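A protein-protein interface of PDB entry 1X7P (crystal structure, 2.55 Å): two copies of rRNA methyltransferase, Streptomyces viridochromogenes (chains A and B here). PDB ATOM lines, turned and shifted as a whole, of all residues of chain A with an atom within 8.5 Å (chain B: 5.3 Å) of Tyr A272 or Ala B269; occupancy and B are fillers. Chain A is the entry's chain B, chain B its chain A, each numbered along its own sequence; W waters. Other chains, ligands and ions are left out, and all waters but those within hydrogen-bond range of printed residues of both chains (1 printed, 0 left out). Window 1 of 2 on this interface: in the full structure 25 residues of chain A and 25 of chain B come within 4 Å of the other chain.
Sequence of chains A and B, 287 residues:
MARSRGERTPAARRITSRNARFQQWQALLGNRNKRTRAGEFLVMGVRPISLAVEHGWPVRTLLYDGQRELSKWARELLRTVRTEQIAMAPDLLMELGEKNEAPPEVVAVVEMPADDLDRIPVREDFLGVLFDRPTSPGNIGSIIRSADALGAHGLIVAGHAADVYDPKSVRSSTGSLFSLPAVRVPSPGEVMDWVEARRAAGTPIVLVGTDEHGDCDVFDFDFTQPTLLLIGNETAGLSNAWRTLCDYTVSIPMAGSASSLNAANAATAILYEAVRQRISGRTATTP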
ATOM      1  N   LEU A 127     -30.158   9.487  -5.329  1.00  0.00           N
ATOM      2  CA  LEU A 127     -29.997  10.803  -5.908  1.00  0.00           C
ATOM      3  C   LEU A 127     -30.543  10.707  -7.318  1.00  0.00           C
ATOM      4  O   LEU A 127     -29.986  10.006  -8.164  1.00  0.00           O
ATOM      5  CB  LEU A 127     -28.534  11.214  -5.934  1.00  0.00           C
ATOM      6  CG  LEU A 127     -28.175  12.687  -5.754  1.00  0.00           C
ATOM      7  CD1 LEU A 127     -26.889  12.977  -6.511  1.00  0.00           C
ATOM      8  CD2 LEU A 127     -29.259  13.619  -6.189  1.00  0.00           C
ATOM      9  N   SER A 146     -24.668  14.751 -17.075  1.00  0.00           N
ATOM     10  CA  SER A 146     -24.285  15.293 -15.780  1.00  0.00           C
ATOM     11  C   SER A 146     -24.677  14.386 -14.638  1.00  0.00           C
ATOM     12  O   SER A 146     -23.901  14.222 -13.706  1.00  0.00           O
ATOM     13  CB  SER A 146     -24.907  16.678 -15.550  1.00  0.00           C
ATOM     14  OG  SER A 146     -24.127  17.689 -16.166  1.00  0.00           O
ATOM     15  N   ALA A 147     -25.875  13.815 -14.681  1.00  0.00           N
ATOM     16  CA  ALA A 147     -26.328  12.929 -13.596  1.00  0.00           C
ATOM     17  C   ALA A 147     -25.515  11.620 -13.571  1.00  0.00           C
ATOM     18  O   ALA A 147     -25.193  11.097 -12.512  1.00  0.00           O
ATOM     19  CB  ALA A 147     -27.832  12.643 -13.716  1.00  0.00           C
ATOM     20  N   LEU A 150     -21.839  12.586 -12.183  1.00  0.00           N
ATOM     21  CA  LEU A 150     -21.757  13.048 -10.810  1.00  0.00           C
ATOM     22  C   LEU A 150     -22.414  12.039  -9.863  1.00  0.00           C
ATOM     23  O   LEU A 150     -22.780  12.367  -8.733  1.00  0.00           O
ATOM     24  CB  LEU A 150     -22.412  14.432 -10.703  1.00  0.00           C
ATOM     25  CG  LEU A 150     -21.601  15.534 -11.392  1.00  0.00           C
ATOM     26  CD1 LEU A 150     -22.425  16.807 -11.591  1.00  0.00           C
ATOM     27  CD2 LEU A 150     -20.353  15.855 -10.622  1.00  0.00           C
ATOM     28  N   GLY A 151     -22.590  10.813 -10.337  1.00  0.00           N
ATOM     29  CA  GLY A 151     -23.123   9.725  -9.520  1.00  0.00           C
ATOM     30  C   GLY A 151     -24.603   9.664  -9.145  1.00  0.00           C
ATOM     31  O   GLY A 151     -24.940   8.917  -8.239  1.00  0.00           O
ATOM     32  N   VAL A 218     -28.813  26.556  -1.669  1.00  0.00           N
ATOM     33  CA  VAL A 218     -28.558  25.186  -2.044  1.00  0.00           C
ATOM     34  C   VAL A 218     -27.517  24.513  -1.131  1.00  0.00           C
ATOM     35  O   VAL A 218     -27.605  23.328  -0.876  1.00  0.00           O
ATOM     36  CB  VAL A 218     -28.195  25.095  -3.551  1.00  0.00           C
ATOM     37  CG1 VAL A 218     -26.867  25.780  -3.844  1.00  0.00           C
ATOM     38  CG2 VAL A 218     -28.190  23.652  -4.014  1.00  0.00           C
ATOM     39  N   PHE A 223     -28.153  17.354   1.337  1.00  0.00           N
ATOM     40  CA  PHE A 223     -28.158  16.408   0.216  1.00  0.00           C
ATOM     41  C   PHE A 223     -27.596  15.007   0.548  1.00  0.00           C
ATOM     42  O   PHE A 223     -27.466  14.195  -0.346  1.00  0.00           O
ATOM     43  CB  PHE A 223     -27.412  17.007  -0.971  1.00  0.00           C
ATOM     44  CG  PHE A 223     -28.176  18.090  -1.686  1.00  0.00           C
ATOM     45  CD1 PHE A 223     -29.220  17.766  -2.553  1.00  0.00           C
ATOM     46  CD2 PHE A 223     -27.837  19.434  -1.520  1.00  0.00           C
ATOM     47  CE1 PHE A 223     -29.920  18.758  -3.232  1.00  0.00           C
ATOM     48  CE2 PHE A 223     -28.527  20.437  -2.203  1.00  0.00           C
ATOM     49  CZ  PHE A 223     -29.570  20.096  -3.061  1.00  0.00           C
ATOM     50  N   LEU A 229     -34.380  15.521  -7.082  1.00  0.00           N
ATOM     51  CA  LEU A 229     -34.197  16.934  -7.408  1.00  0.00           C
ATOM     52  C   LEU A 229     -35.080  17.342  -8.595  1.00  0.00           C
ATOM     53  O   LEU A 229     -34.913  16.828  -9.688  1.00  0.00           O
ATOM     54  CB  LEU A 229     -32.735  17.169  -7.754  1.00  0.00           C
ATOM     55  CG  LEU A 229     -32.316  18.622  -7.878  1.00  0.00           C
ATOM     56  CD1 LEU A 229     -32.176  19.269  -6.491  1.00  0.00           C
ATOM     57  CD2 LEU A 229     -31.011  18.703  -8.650  1.00  0.00           C
ATOM     58  N   ILE A 252     -29.599  28.627  -6.105  1.00  0.00           N
ATOM     59  CA  ILE A 252     -28.221  29.044  -6.239  1.00  0.00           C
ATOM     60  C   ILE A 252     -28.176  30.555  -6.202  1.00  0.00           C
ATOM     61  O   ILE A 252     -28.789  31.184  -7.056  1.00  0.00           O
ATOM     62  CB  ILE A 252     -27.665  28.588  -7.602  1.00  0.00           C
ATOM     63  CG1 ILE A 252     -27.809  27.079  -7.767  1.00  0.00           C
ATOM     64  CG2 ILE A 252     -26.199  29.051  -7.760  1.00  0.00           C
ATOM     65  CD1 ILE A 252     -27.644  26.617  -9.186  1.00  0.00           C
ATOM     66  N   LEU A 261     -30.079  31.036 -14.699  1.00  0.00           N
ATOM     67  CA  LEU A 261     -29.330  29.921 -15.286  1.00  0.00           C
ATOM     68  C   LEU A 261     -30.163  29.011 -16.198  1.00  0.00           C
ATOM     69  O   LEU A 261     -31.361  28.818 -15.993  1.00  0.00           O
ATOM     70  CB  LEU A 261     -28.713  29.049 -14.192  1.00  0.00           C
ATOM     71  CG  LEU A 261     -27.591  29.622 -13.321  1.00  0.00           C
ATOM     72  CD1 LEU A 261     -27.207  28.600 -12.242  1.00  0.00           C
ATOM     73  CD2 LEU A 261     -26.390  29.995 -14.142  1.00  0.00           C
ATOM     74  N   ALA A 264     -29.902  22.834 -17.594  1.00  0.00           N
ATOM     75  CA  ALA A 264     -28.827  21.856 -17.517  1.00  0.00           C
ATOM     76  C   ALA A 264     -27.625  22.317 -16.701  1.00  0.00           C
ATOM     77  O   ALA A 264     -27.017  21.505 -16.010  1.00  0.00           O
ATOM     78  CB  ALA A 264     -28.380  21.433 -18.911  1.00  0.00           C
ATOM     79  N   ASN A 265     -27.285  23.599 -16.804  1.00  0.00           N
ATOM     80  CA  ASN A 265     -26.172  24.183 -16.067  1.00  0.00           C
ATOM     81  C   ASN A 265     -26.471  24.275 -14.579  1.00  0.00           C
ATOM     82  O   ASN A 265     -25.624  23.966 -13.738  1.00  0.00           O
ATOM     83  CB  ASN A 265     -25.878  25.598 -16.567  1.00  0.00           C
ATOM     84  CG  ASN A 265     -25.307  25.623 -17.949  1.00  0.00           C
ATOM     85  OD1 ASN A 265     -25.465  26.602 -18.680  1.00  0.00           O
ATOM     86  ND2 ASN A 265     -24.631  24.555 -18.321  1.00  0.00           N
ATOM     87  N   ALA A 266     -27.682  24.734 -14.271  1.00  0.00           N
ATOM     88  CA  ALA A 266     -28.118  24.890 -12.901  1.00  0.00           C
ATOM     89  C   ALA A 266     -28.133  23.536 -12.208  1.00  0.00           C
ATOM     90  O   ALA A 266     -27.717  23.405 -11.039  1.00  0.00           O
ATOM     91  CB  ALA A 266     -29.494  25.511 -12.872  1.00  0.00           C
ATOM     92  N   ALA A 267     -28.602  22.528 -12.942  1.00  0.00           N
ATOM     93  CA  ALA A 267     -28.830  21.195 -12.381  1.00  0.00           C
ATOM     94  C   ALA A 267     -27.497  20.507 -12.133  1.00  0.00           C
ATOM     95  O   ALA A 267     -27.314  19.844 -11.111  1.00  0.00           O
ATOM     96  CB  ALA A 267     -29.714  20.352 -13.330  1.00  0.00           C
ATOM     97  N   THR A 268     -26.570  20.688 -13.073  1.00  0.00           N
ATOM     98  CA  THR A 268     -25.190  20.249 -12.925  1.00  0.00           C
ATOM     99  C   THR A 268     -24.557  20.776 -11.632  1.00  0.00           C
ATOM    100  O   THR A 268     -23.955  20.000 -10.897  1.00  0.00           O
ATOM    101  CB  THR A 268     -24.366  20.733 -14.114  1.00  0.00           C
ATOM    102  OG1 THR A 268     -24.792  20.071 -15.308  1.00  0.00           O
ATOM    103  CG2 THR A 268     -22.889  20.342 -13.959  1.00  0.00           C
ATOM    104  N   ALA A 269     -24.734  22.071 -11.362  1.00  0.00           N
ATOM    105  CA  ALA A 269     -24.174  22.736 -10.197  1.00  0.00           C
ATOM    106  C   ALA A 269     -24.757  22.224  -8.870  1.00  0.00           C
ATOM    107  O   ALA A 269     -24.029  22.116  -7.869  1.00  0.00           O
ATOM    108  CB  ALA A 269     -24.370  24.276 -10.321  1.00  0.00           C
ATOM    109  N   ILE A 270     -26.049  21.884  -8.864  1.00  0.00           N
ATOM    110  CA  ILE A 270     -26.732  21.394  -7.657  1.00  0.00           C
ATOM    111  C   ILE A 270     -26.336  19.940  -7.398  1.00  0.00           C
ATOM    112  O   ILE A 270     -25.995  19.557  -6.288  1.00  0.00           O
ATOM    113  CB  ILE A 270     -28.262  21.515  -7.805  1.00  0.00           C
ATOM    114  CG1 ILE A 270     -28.676  22.977  -7.968  1.00  0.00           C
ATOM    115  CG2 ILE A 270     -28.969  20.930  -6.605  1.00  0.00           C
ATOM    116  CD1 ILE A 270     -30.138  23.196  -8.327  1.00  0.00           C
ATOM    117  N   LEU A 271     -26.395  19.123  -8.439  1.00  0.00           N
ATOM    118  CA  LEU A 271     -25.846  17.781  -8.375  1.00  0.00           C
ATOM    119  C   LEU A 271     -24.403  17.825  -7.844  1.00  0.00           C
ATOM    120  O   LEU A 271     -24.016  16.983  -7.032  1.00  0.00           O
ATOM    121  CB  LEU A 271     -25.874  17.148  -9.758  1.00  0.00           C
ATOM    122  CG  LEU A 271     -26.916  16.084 -10.151  1.00  0.00           C
ATOM    123  CD1 LEU A 271     -28.049  15.866  -9.149  1.00  0.00           C
ATOM    124  CD2 LEU A 271     -27.428  16.394 -11.529  1.00  0.00           C
ATOM    125  N   TYR A 272     -23.612  18.805  -8.283  1.00  0.00           N
ATOM    126  CA  TYR A 272     -22.238  18.893  -7.814  1.00  0.00           C
ATOM    127  C   TYR A 272     -22.203  19.202  -6.312  1.00  0.00           C
ATOM    128  O   TYR A 272     -21.411  18.628  -5.582  1.00  0.00           O
ATOM    129  CB  TYR A 272     -21.417  19.952  -8.564  1.00  0.00           C
ATOM    130  CG  TYR A 272     -20.313  20.496  -7.685  1.00  0.00           C
ATOM    131  CD1 TYR A 272     -19.245  19.694  -7.344  1.00  0.00           C
ATOM    132  CD2 TYR A 272     -20.351  21.797  -7.180  1.00  0.00           C
ATOM    133  CE1 TYR A 272     -18.220  20.165  -6.503  1.00  0.00           C
ATOM    134  CE2 TYR A 272     -19.338  22.277  -6.354  1.00  0.00           C
ATOM    135  CZ  TYR A 272     -18.276  21.439  -6.008  1.00  0.00           C
ATOM    136  OH  TYR A 272     -17.251  21.844  -5.190  1.00  0.00           O
ATOM    137  N   GLU A 273     -23.046  20.122  -5.859  1.00  0.00           N
ATOM    138  CA  GLU A 273     -23.145  20.430  -4.423  1.00  0.00           C
ATOM    139  C   GLU A 273     -23.463  19.195  -3.599  1.00  0.00           C
ATOM    140  O   GLU A 273     -23.008  19.055  -2.461  1.00  0.00           O
ATOM    141  CB  GLU A 273     -24.234  21.477  -4.179  1.00  0.00           C
ATOM    142  CG  GLU A 273     -24.582  21.710  -2.707  1.00  0.00           C
ATOM    143  CD  GLU A 273     -23.443  22.280  -1.899  1.00  0.00           C
ATOM    144  OE1 GLU A 273     -22.467  22.826  -2.498  1.00  0.00           O
ATOM    145  OE2 GLU A 273     -23.528  22.188  -0.652  1.00  0.00           O
ATOM    146  N   ALA A 274     -24.281  18.315  -4.171  1.00  0.00           N
ATOM    147  CA  ALA A 274     -24.710  17.105  -3.471  1.00  0.00           C
ATOM    148  C   ALA A 274     -23.511  16.213  -3.293  1.00  0.00           C
ATOM    149  O   ALA A 274     -23.284  15.716  -2.200  1.00  0.00           O
ATOM    150  CB  ALA A 274     -25.811  16.371  -4.243  1.00  0.00           C
ATOM    151  N   VAL A 275     -22.742  16.034  -4.363  1.00  0.00           N
ATOM    152  CA  VAL A 275     -21.558  15.198  -4.331  1.00  0.00           C
ATOM    153  C   VAL A 275     -20.610  15.768  -3.299  1.00  0.00           C
ATOM    154  O   VAL A 275     -19.978  15.018  -2.580  1.00  0.00           O
ATOM    155  CB  VAL A 275     -20.795  15.156  -5.699  1.00  0.00           C
ATOM    156  CG1 VAL A 275     -19.488  14.428  -5.558  1.00  0.00           C
ATOM    157  CG2 VAL A 275     -21.628  14.475  -6.789  1.00  0.00           C
ATOM    158  N   ARG A 276     -20.497  17.093  -3.234  1.00  0.00           N
ATOM    159  CA  ARG A 276     -19.526  17.702  -2.343  1.00  0.00           C
ATOM    160  C   ARG A 276     -19.870  17.429  -0.903  1.00  0.00           C
ATOM    161  O   ARG A 276     -18.992  17.173  -0.107  1.00  0.00           O
ATOM    162  CB  ARG A 276     -19.443  19.197  -2.572  1.00  0.00           C
ATOM    163  CG  ARG A 276     -18.491  19.925  -1.635  1.00  0.00           C
ATOM    164  CD  ARG A 276     -18.672  21.442  -1.662  1.00  0.00           C
ATOM    165  NE  ARG A 276     -19.834  21.908  -0.906  1.00  0.00           N
ATOM    166  CZ  ARG A 276     -19.863  22.045   0.428  1.00  0.00           C
ATOM    167  NH1 ARG A 276     -18.802  21.746   1.165  1.00  0.00           N
ATOM    168  NH2 ARG A 276     -20.954  22.490   1.023  1.00  0.00           N
ATOM    169  N   GLN A 277     -21.143  17.499  -0.563  1.00  0.00           N
ATOM    170  CA  GLN A 277     -21.554  17.271   0.814  1.00  0.00           C
ATOM    171  C   GLN A 277     -21.317  15.828   1.152  1.00  0.00           C
ATOM    172  O   GLN A 277     -20.820  15.519   2.222  1.00  0.00           O
ATOM    173  CB  GLN A 277     -23.029  17.612   1.044  1.00  0.00           C
ATOM    174  CG  GLN A 277     -23.329  19.089   1.103  1.00  0.00           C
ATOM    175  CD  GLN A 277     -24.809  19.359   1.271  1.00  0.00           C
ATOM    176  OE1 GLN A 277     -25.517  18.568   1.912  1.00  0.00           O
ATOM    177  NE2 GLN A 277     -25.280  20.474   0.723  1.00  0.00           N
ATOM    178  N   ARG A 278     -21.688  14.949   0.229  1.00  0.00           N
ATOM    179  CA  ARG A 278     -21.608  13.511   0.455  1.00  0.00           C
ATOM    180  C   ARG A 278     -20.166  13.076   0.669  1.00  0.00           C
ATOM    181  O   ARG A 278     -19.876  12.239   1.513  1.00  0.00           O
ATOM    182  CB  ARG A 278     -22.248  12.754  -0.719  1.00  0.00           C
ATOM    183  CG  ARG A 278     -23.760  12.654  -0.603  1.00  0.00           C
ATOM    184  CD  ARG A 278     -24.460  12.190  -1.859  1.00  0.00           C
ATOM    185  NE  ARG A 278     -25.904  12.319  -1.718  1.00  0.00           N
ATOM    186  CZ  ARG A 278     -26.800  11.420  -2.138  1.00  0.00           C
ATOM    187  NH1 ARG A 278     -26.422  10.318  -2.764  1.00  0.00           N
ATOM    188  NH2 ARG A 278     -28.100  11.623  -1.924  1.00  0.00           N
ATOM    189  N   ILE A 279     -19.263  13.680  -0.082  1.00  0.00           N
ATOM    190  CA  ILE A 279     -17.837  13.468   0.104  1.00  0.00           C
ATOM    191  C   ILE A 279     -17.282  14.178   1.336  1.00  0.00           C
ATOM    192  O   ILE A 279     -16.462  13.586   2.030  1.00  0.00           O
ATOM    193  CB  ILE A 279     -17.058  13.836  -1.177  1.00  0.00           C
ATOM    194  CG1 ILE A 279     -17.460  12.874  -2.288  1.00  0.00           C
ATOM    195  CG2 ILE A 279     -15.540  13.771  -0.947  1.00  0.00           C
ATOM    196  CD1 ILE A 279     -16.923  13.233  -3.637  1.00  0.00           C
ATOM    197  N   VAL B 218     -11.838  20.698  -6.628  1.00  0.00           N
ATOM    198  CA  VAL B 218     -12.316  22.072  -6.728  1.00  0.00           C
ATOM    199  C   VAL B 218     -12.696  22.699  -5.362  1.00  0.00           C
ATOM    200  O   VAL B 218     -12.499  23.902  -5.162  1.00  0.00           O
ATOM    201  CB  VAL B 218     -13.507  22.109  -7.722  1.00  0.00           C
ATOM    202  CG1 VAL B 218     -14.755  21.525  -7.099  1.00  0.00           C
ATOM    203  CG2 VAL B 218     -13.762  23.462  -8.195  1.00  0.00           C
ATOM    204  N   PHE B 219     -13.223  21.880  -4.447  1.00  0.00           N
ATOM    205  CA  PHE B 219     -13.605  22.321  -3.111  1.00  0.00           C
ATOM    206  C   PHE B 219     -12.417  22.358  -2.132  1.00  0.00           C
ATOM    207  O   PHE B 219     -12.544  22.866  -1.028  1.00  0.00           O
ATOM    208  CB  PHE B 219     -14.754  21.453  -2.528  1.00  0.00           C
ATOM    209  CG  PHE B 219     -14.480  19.952  -2.532  1.00  0.00           C
ATOM    210  CD1 PHE B 219     -15.068  19.121  -3.499  1.00  0.00           C
ATOM    211  CD2 PHE B 219     -13.654  19.369  -1.576  1.00  0.00           C
ATOM    212  CE1 PHE B 219     -14.823  17.747  -3.509  1.00  0.00           C
ATOM    213  CE2 PHE B 219     -13.403  17.991  -1.587  1.00  0.00           C
ATOM    214  CZ  PHE B 219     -13.985  17.182  -2.547  1.00  0.00           C
ATOM    215  N   ILE B 252     -13.607  18.616 -10.802  1.00  0.00           N
ATOM    216  CA  ILE B 252     -14.828  18.024 -10.277  1.00  0.00           C
ATOM    217  C   ILE B 252     -14.648  16.517 -10.212  1.00  0.00           C
ATOM    218  O   ILE B 252     -14.462  15.901 -11.243  1.00  0.00           O
ATOM    219  CB  ILE B 252     -16.046  18.331 -11.193  1.00  0.00           C
ATOM    220  CG1 ILE B 252     -16.145  19.807 -11.536  1.00  0.00           C
ATOM    221  CG2 ILE B 252     -17.339  17.903 -10.542  1.00  0.00           C
ATOM    222  CD1 ILE B 252     -15.991  20.684 -10.340  1.00  0.00           C
ATOM    223  N   PRO B 253     -14.740  15.897  -9.038  1.00  0.00           N
ATOM    224  CA  PRO B 253     -14.710  14.419  -8.977  1.00  0.00           C
ATOM    225  C   PRO B 253     -15.895  13.777  -9.718  1.00  0.00           C
ATOM    226  O   PRO B 253     -17.000  14.329  -9.695  1.00  0.00           O
ATOM    227  CB  PRO B 253     -14.803  14.111  -7.479  1.00  0.00           C
ATOM    228  CG  PRO B 253     -15.350  15.305  -6.848  1.00  0.00           C
ATOM    229  CD  PRO B 253     -14.925  16.502  -7.703  1.00  0.00           C
ATOM    230  N   ALA B 264     -19.652  23.912 -20.527  1.00  0.00           N
ATOM    231  CA  ALA B 264     -20.460  24.947 -19.888  1.00  0.00           C
ATOM    232  C   ALA B 264     -20.993  24.469 -18.556  1.00  0.00           C
ATOM    233  O   ALA B 264     -21.026  25.242 -17.591  1.00  0.00           O
ATOM    234  CB  ALA B 264     -21.622  25.406 -20.799  1.00  0.00           C
ATOM    235  N   ASN B 265     -21.421  23.212 -18.506  1.00  0.00           N
ATOM    236  CA  ASN B 265     -21.912  22.613 -17.278  1.00  0.00           C
ATOM    237  C   ASN B 265     -20.807  22.581 -16.260  1.00  0.00           C
ATOM    238  O   ASN B 265     -21.029  22.916 -15.121  1.00  0.00           O
ATOM    239  CB  ASN B 265     -22.423  21.188 -17.515  1.00  0.00           C
ATOM    240  CG  ASN B 265     -23.701  21.150 -18.349  1.00  0.00           C
ATOM    241  OD1 ASN B 265     -23.934  20.205 -19.105  1.00  0.00           O
ATOM    242  ND2 ASN B 265     -24.522  22.181 -18.222  1.00  0.00           N
ATOM    243  N   ALA B 266     -19.595  22.219 -16.688  1.00  0.00           N
ATOM    244  CA  ALA B 266     -18.476  22.099 -15.776  1.00  0.00           C
ATOM    245  C   ALA B 266     -18.140  23.464 -15.249  1.00  0.00           C
ATOM    246  O   ALA B 266     -17.868  23.628 -14.064  1.00  0.00           O
ATOM    247  CB  ALA B 266     -17.263  21.489 -16.468  1.00  0.00           C
ATOM    248  N   ALA B 267     -18.178  24.446 -16.138  1.00  0.00           N
ATOM    249  CA  ALA B 267     -17.768  25.783 -15.808  1.00  0.00           C
ATOM    250  C   ALA B 267     -18.764  26.397 -14.834  1.00  0.00           C
ATOM    251  O   ALA B 267     -18.396  27.175 -13.950  1.00  0.00           O
ATOM    252  CB  ALA B 267     -17.690  26.602 -17.062  1.00  0.00           C
ATOM    253  N   THR B 268     -20.033  26.028 -14.993  1.00  0.00           N
ATOM    254  CA  THR B 268     -21.069  26.489 -14.082  1.00  0.00           C
ATOM    255  C   THR B 268     -20.870  25.885 -12.706  1.00  0.00           C
ATOM    256  O   THR B 268     -20.998  26.587 -11.707  1.00  0.00           O
ATOM    257  CB  THR B 268     -22.471  26.122 -14.606  1.00  0.00           C
ATOM    258  OG1 THR B 268     -22.636  26.649 -15.930  1.00  0.00           O
ATOM    259  CG2 THR B 268     -23.580  26.773 -13.735  1.00  0.00           C
ATOM    260  N   ALA B 269     -20.553  24.594 -12.643  1.00  0.00           N
ATOM    261  CA  ALA B 269     -20.327  23.953 -11.353  1.00  0.00           C
ATOM    262  C   ALA B 269     -19.196  24.631 -10.566  1.00  0.00           C
ATOM    263  O   ALA B 269     -19.305  24.802  -9.348  1.00  0.00           O
ATOM    264  CB  ALA B 269     -20.043  22.483 -11.533  1.00  0.00           C
ATOM    265  N   ILE B 270     -18.141  25.046 -11.267  1.00  0.00           N
ATOM    266  CA  ILE B 270     -16.931  25.541 -10.623  1.00  0.00           C
ATOM    267  C   ILE B 270     -17.065  27.017 -10.273  1.00  0.00           C
ATOM    268  O   ILE B 270     -16.626  27.443  -9.228  1.00  0.00           O
ATOM    269  CB  ILE B 270     -15.690  25.275 -11.506  1.00  0.00           C
ATOM    270  CG1 ILE B 270     -15.453  23.760 -11.685  1.00  0.00           C
ATOM    271  CG2 ILE B 270     -14.459  25.889 -10.893  1.00  0.00           C
ATOM    272  CD1 ILE B 270     -14.511  23.382 -12.838  1.00  0.00           C
ATOM    273  N   LEU B 271     -17.650  27.801 -11.154  1.00  0.00           N
ATOM    274  CA  LEU B 271     -18.081  29.147 -10.807  1.00  0.00           C
ATOM    275  C   LEU B 271     -18.973  29.112  -9.573  1.00  0.00           C
ATOM    276  O   LEU B 271     -18.798  29.899  -8.681  1.00  0.00           O
ATOM    277  CB  LEU B 271     -18.871  29.780 -11.951  1.00  0.00           C
ATOM    278  CG  LEU B 271     -18.245  30.768 -12.932  1.00  0.00           C
ATOM    279  CD1 LEU B 271     -16.735  31.007 -12.771  1.00  0.00           C
ATOM    280  CD2 LEU B 271     -18.600  30.333 -14.375  1.00  0.00           C
ATOM    281  N   TYR B 272     -19.930  28.203  -9.515  1.00  0.00           N
ATOM    282  CA  TYR B 272     -20.769  28.073  -8.318  1.00  0.00           C
ATOM    283  C   TYR B 272     -19.921  27.810  -7.060  1.00  0.00           C
ATOM    284  O   TYR B 272     -20.218  28.342  -5.993  1.00  0.00           O
ATOM    285  CB  TYR B 272     -21.847  26.971  -8.459  1.00  0.00           C
ATOM    286  CG  TYR B 272     -22.296  26.490  -7.106  1.00  0.00           C
ATOM    287  CD1 TYR B 272     -23.187  27.236  -6.342  1.00  0.00           C
ATOM    288  CD2 TYR B 272     -21.774  25.338  -6.550  1.00  0.00           C
ATOM    289  CE1 TYR B 272     -23.567  26.808  -5.052  1.00  0.00           C
ATOM    290  CE2 TYR B 272     -22.130  24.920  -5.292  1.00  0.00           C
ATOM    291  CZ  TYR B 272     -23.027  25.648  -4.539  1.00  0.00           C
ATOM    292  OH  TYR B 272     -23.377  25.222  -3.269  1.00  0.00           O
ATOM    293  N   GLU B 273     -18.893  26.978  -7.178  1.00  0.00           N
ATOM    294  CA  GLU B 273     -18.036  26.651  -6.042  1.00  0.00           C
ATOM    295  C   GLU B 273     -17.309  27.878  -5.548  1.00  0.00           C
ATOM    296  O   GLU B 273     -17.219  28.097  -4.347  1.00  0.00           O
ATOM    297  CB  GLU B 273     -17.036  25.566  -6.416  1.00  0.00           C
ATOM    298  CG  GLU B 273     -16.004  25.232  -5.342  1.00  0.00           C
ATOM    299  CD  GLU B 273     -16.573  24.707  -4.025  1.00  0.00           C
ATOM    300  OE1 GLU B 273     -17.675  24.087  -3.967  1.00  0.00           O
ATOM    301  OE2 GLU B 273     -15.859  24.896  -3.021  1.00  0.00           O
HETATM  302  O   HOH W   1     -22.566  17.697 -18.787  1.00  0.00           O
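The side-chain amide nitrogen (ND2) of Asn B265 sits close to the backbone NH (N) of Asn A265 (3.4 Å).
The side-chain amide nitrogen (ND2) of Asn B265 lies within hydrogen-bond range of the backbone carbonyl oxygen (O) of Ala A264 (3.4 Å).
OH of Tyr B272 sits at hydrogen-bond distance from OE1 of Glu A273, 2.7 Å away.
OH of Tyr A272 lies within hydrogen-bond range of OE1 of Glu B273, 2.6 Å away.
Hydrophobic or aromatic side chains of chain B within 4 Å of the printed part of chain A: Val B218, Phe B219, Ile B252, Ala B264 and Tyr B272.
Of the 26 printed residues of chain A, 10 touch a printed residue of chain B.
Printed residues of chain A that touch a printed residue of chain B: Ser A146, Leu A150, Val A218, Ile A252, Ala A264, Asn A265, Thr A268, Tyr A272, Glu A273 and Arg A276.
Among the printed residues, 18 pairs touch across the chains.
Among the printed residues, no Asp or Glu carboxylate lies within 4 Å of a Lys or Arg side-chain nitrogen of the other chain.
Ile A252 touches Tyr B272, but with the chains exchanged Tyr A272 does not touch Ile B252 (4.1 Å).
Ala A264 touches Asn B265, and with the chains exchanged Asn A265 touches Ala B264.
Asn A265 touches Thr B268, and with the chains exchanged Thr A268 touches Asn B265.
Tyr B272 touches its own counterpart, Tyr A272.
Positions printed for both chains: 218, 252, 264, 265, 266, 267, 268, 269, 270, 271, 272 and 273.
Tyr A272 touches just these residues of chain B: Val B218 (3.2 Å), Phe B219 (3.7 Å), Ala B269 (3.9 Å), Tyr B272 (3.9 Å) and Glu B273 (2.6 Å).
Of chain A, only Tyr A272 (3.9 Å) comes within 4 Å of Ala B269.
Of the printed residues of chain A, Thr B268 touches Asn A265 (3.5 Å).
Of the printed residues of chain A, Ala B264 touches Asn A265 (3.6 Å).
Of the printed residues of chain B, Ile A252 touches Tyr B272 (3.8 Å).
Of the printed residues of chain A, Val B218 touches Tyr A272.
The nearest residue of chain A that does not touch Ala B269 is Ala A269 (4.2 Å).
Among the printed residues, pairs that only touch across the chains: Tyr A272 with Val B218, Thr A268 with Asn B265, Asn A265 with Thr B268, Val A218 with Tyr B272, Leu A150 with Ile B252, Asn A265 with Ala B264, Arg A276 with Glu B273, Tyr A272 with Phe B219, Ile A252 with Tyr B272, Leu A150 with Pro B253, Tyr A272 with Ala B269, Tyr A272 with Tyr B272, Ser A146 with Asn B265 and Arg A276 with Phe B219.
Water W1 lies within hydrogen-bond range of OD1 of Asn B265 (2.9 Å) and OG of Ser A146 (3.1 Å).
The side-chain hydroxyl (OG) of Ser A146 is in hydrogen-bond range of the side-chain hydroxyl (OG1) of Thr A268, 2.6 Å away.
The backbone carbonyl oxygen (O) of Ala B264 sits at hydrogen-bond distance from the side-chain hydroxyl (OG1) of Thr B268 (2.7 Å).
OE2 of Glu A273 is in salt-bridge range of NH2 of Arg A276, at 3.1 Å.
The side-chain amide nitrogen of Gln A277 is in hydrogen-bond range of the side-chain carboxylate of Glu A273, 2.8 Å away.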
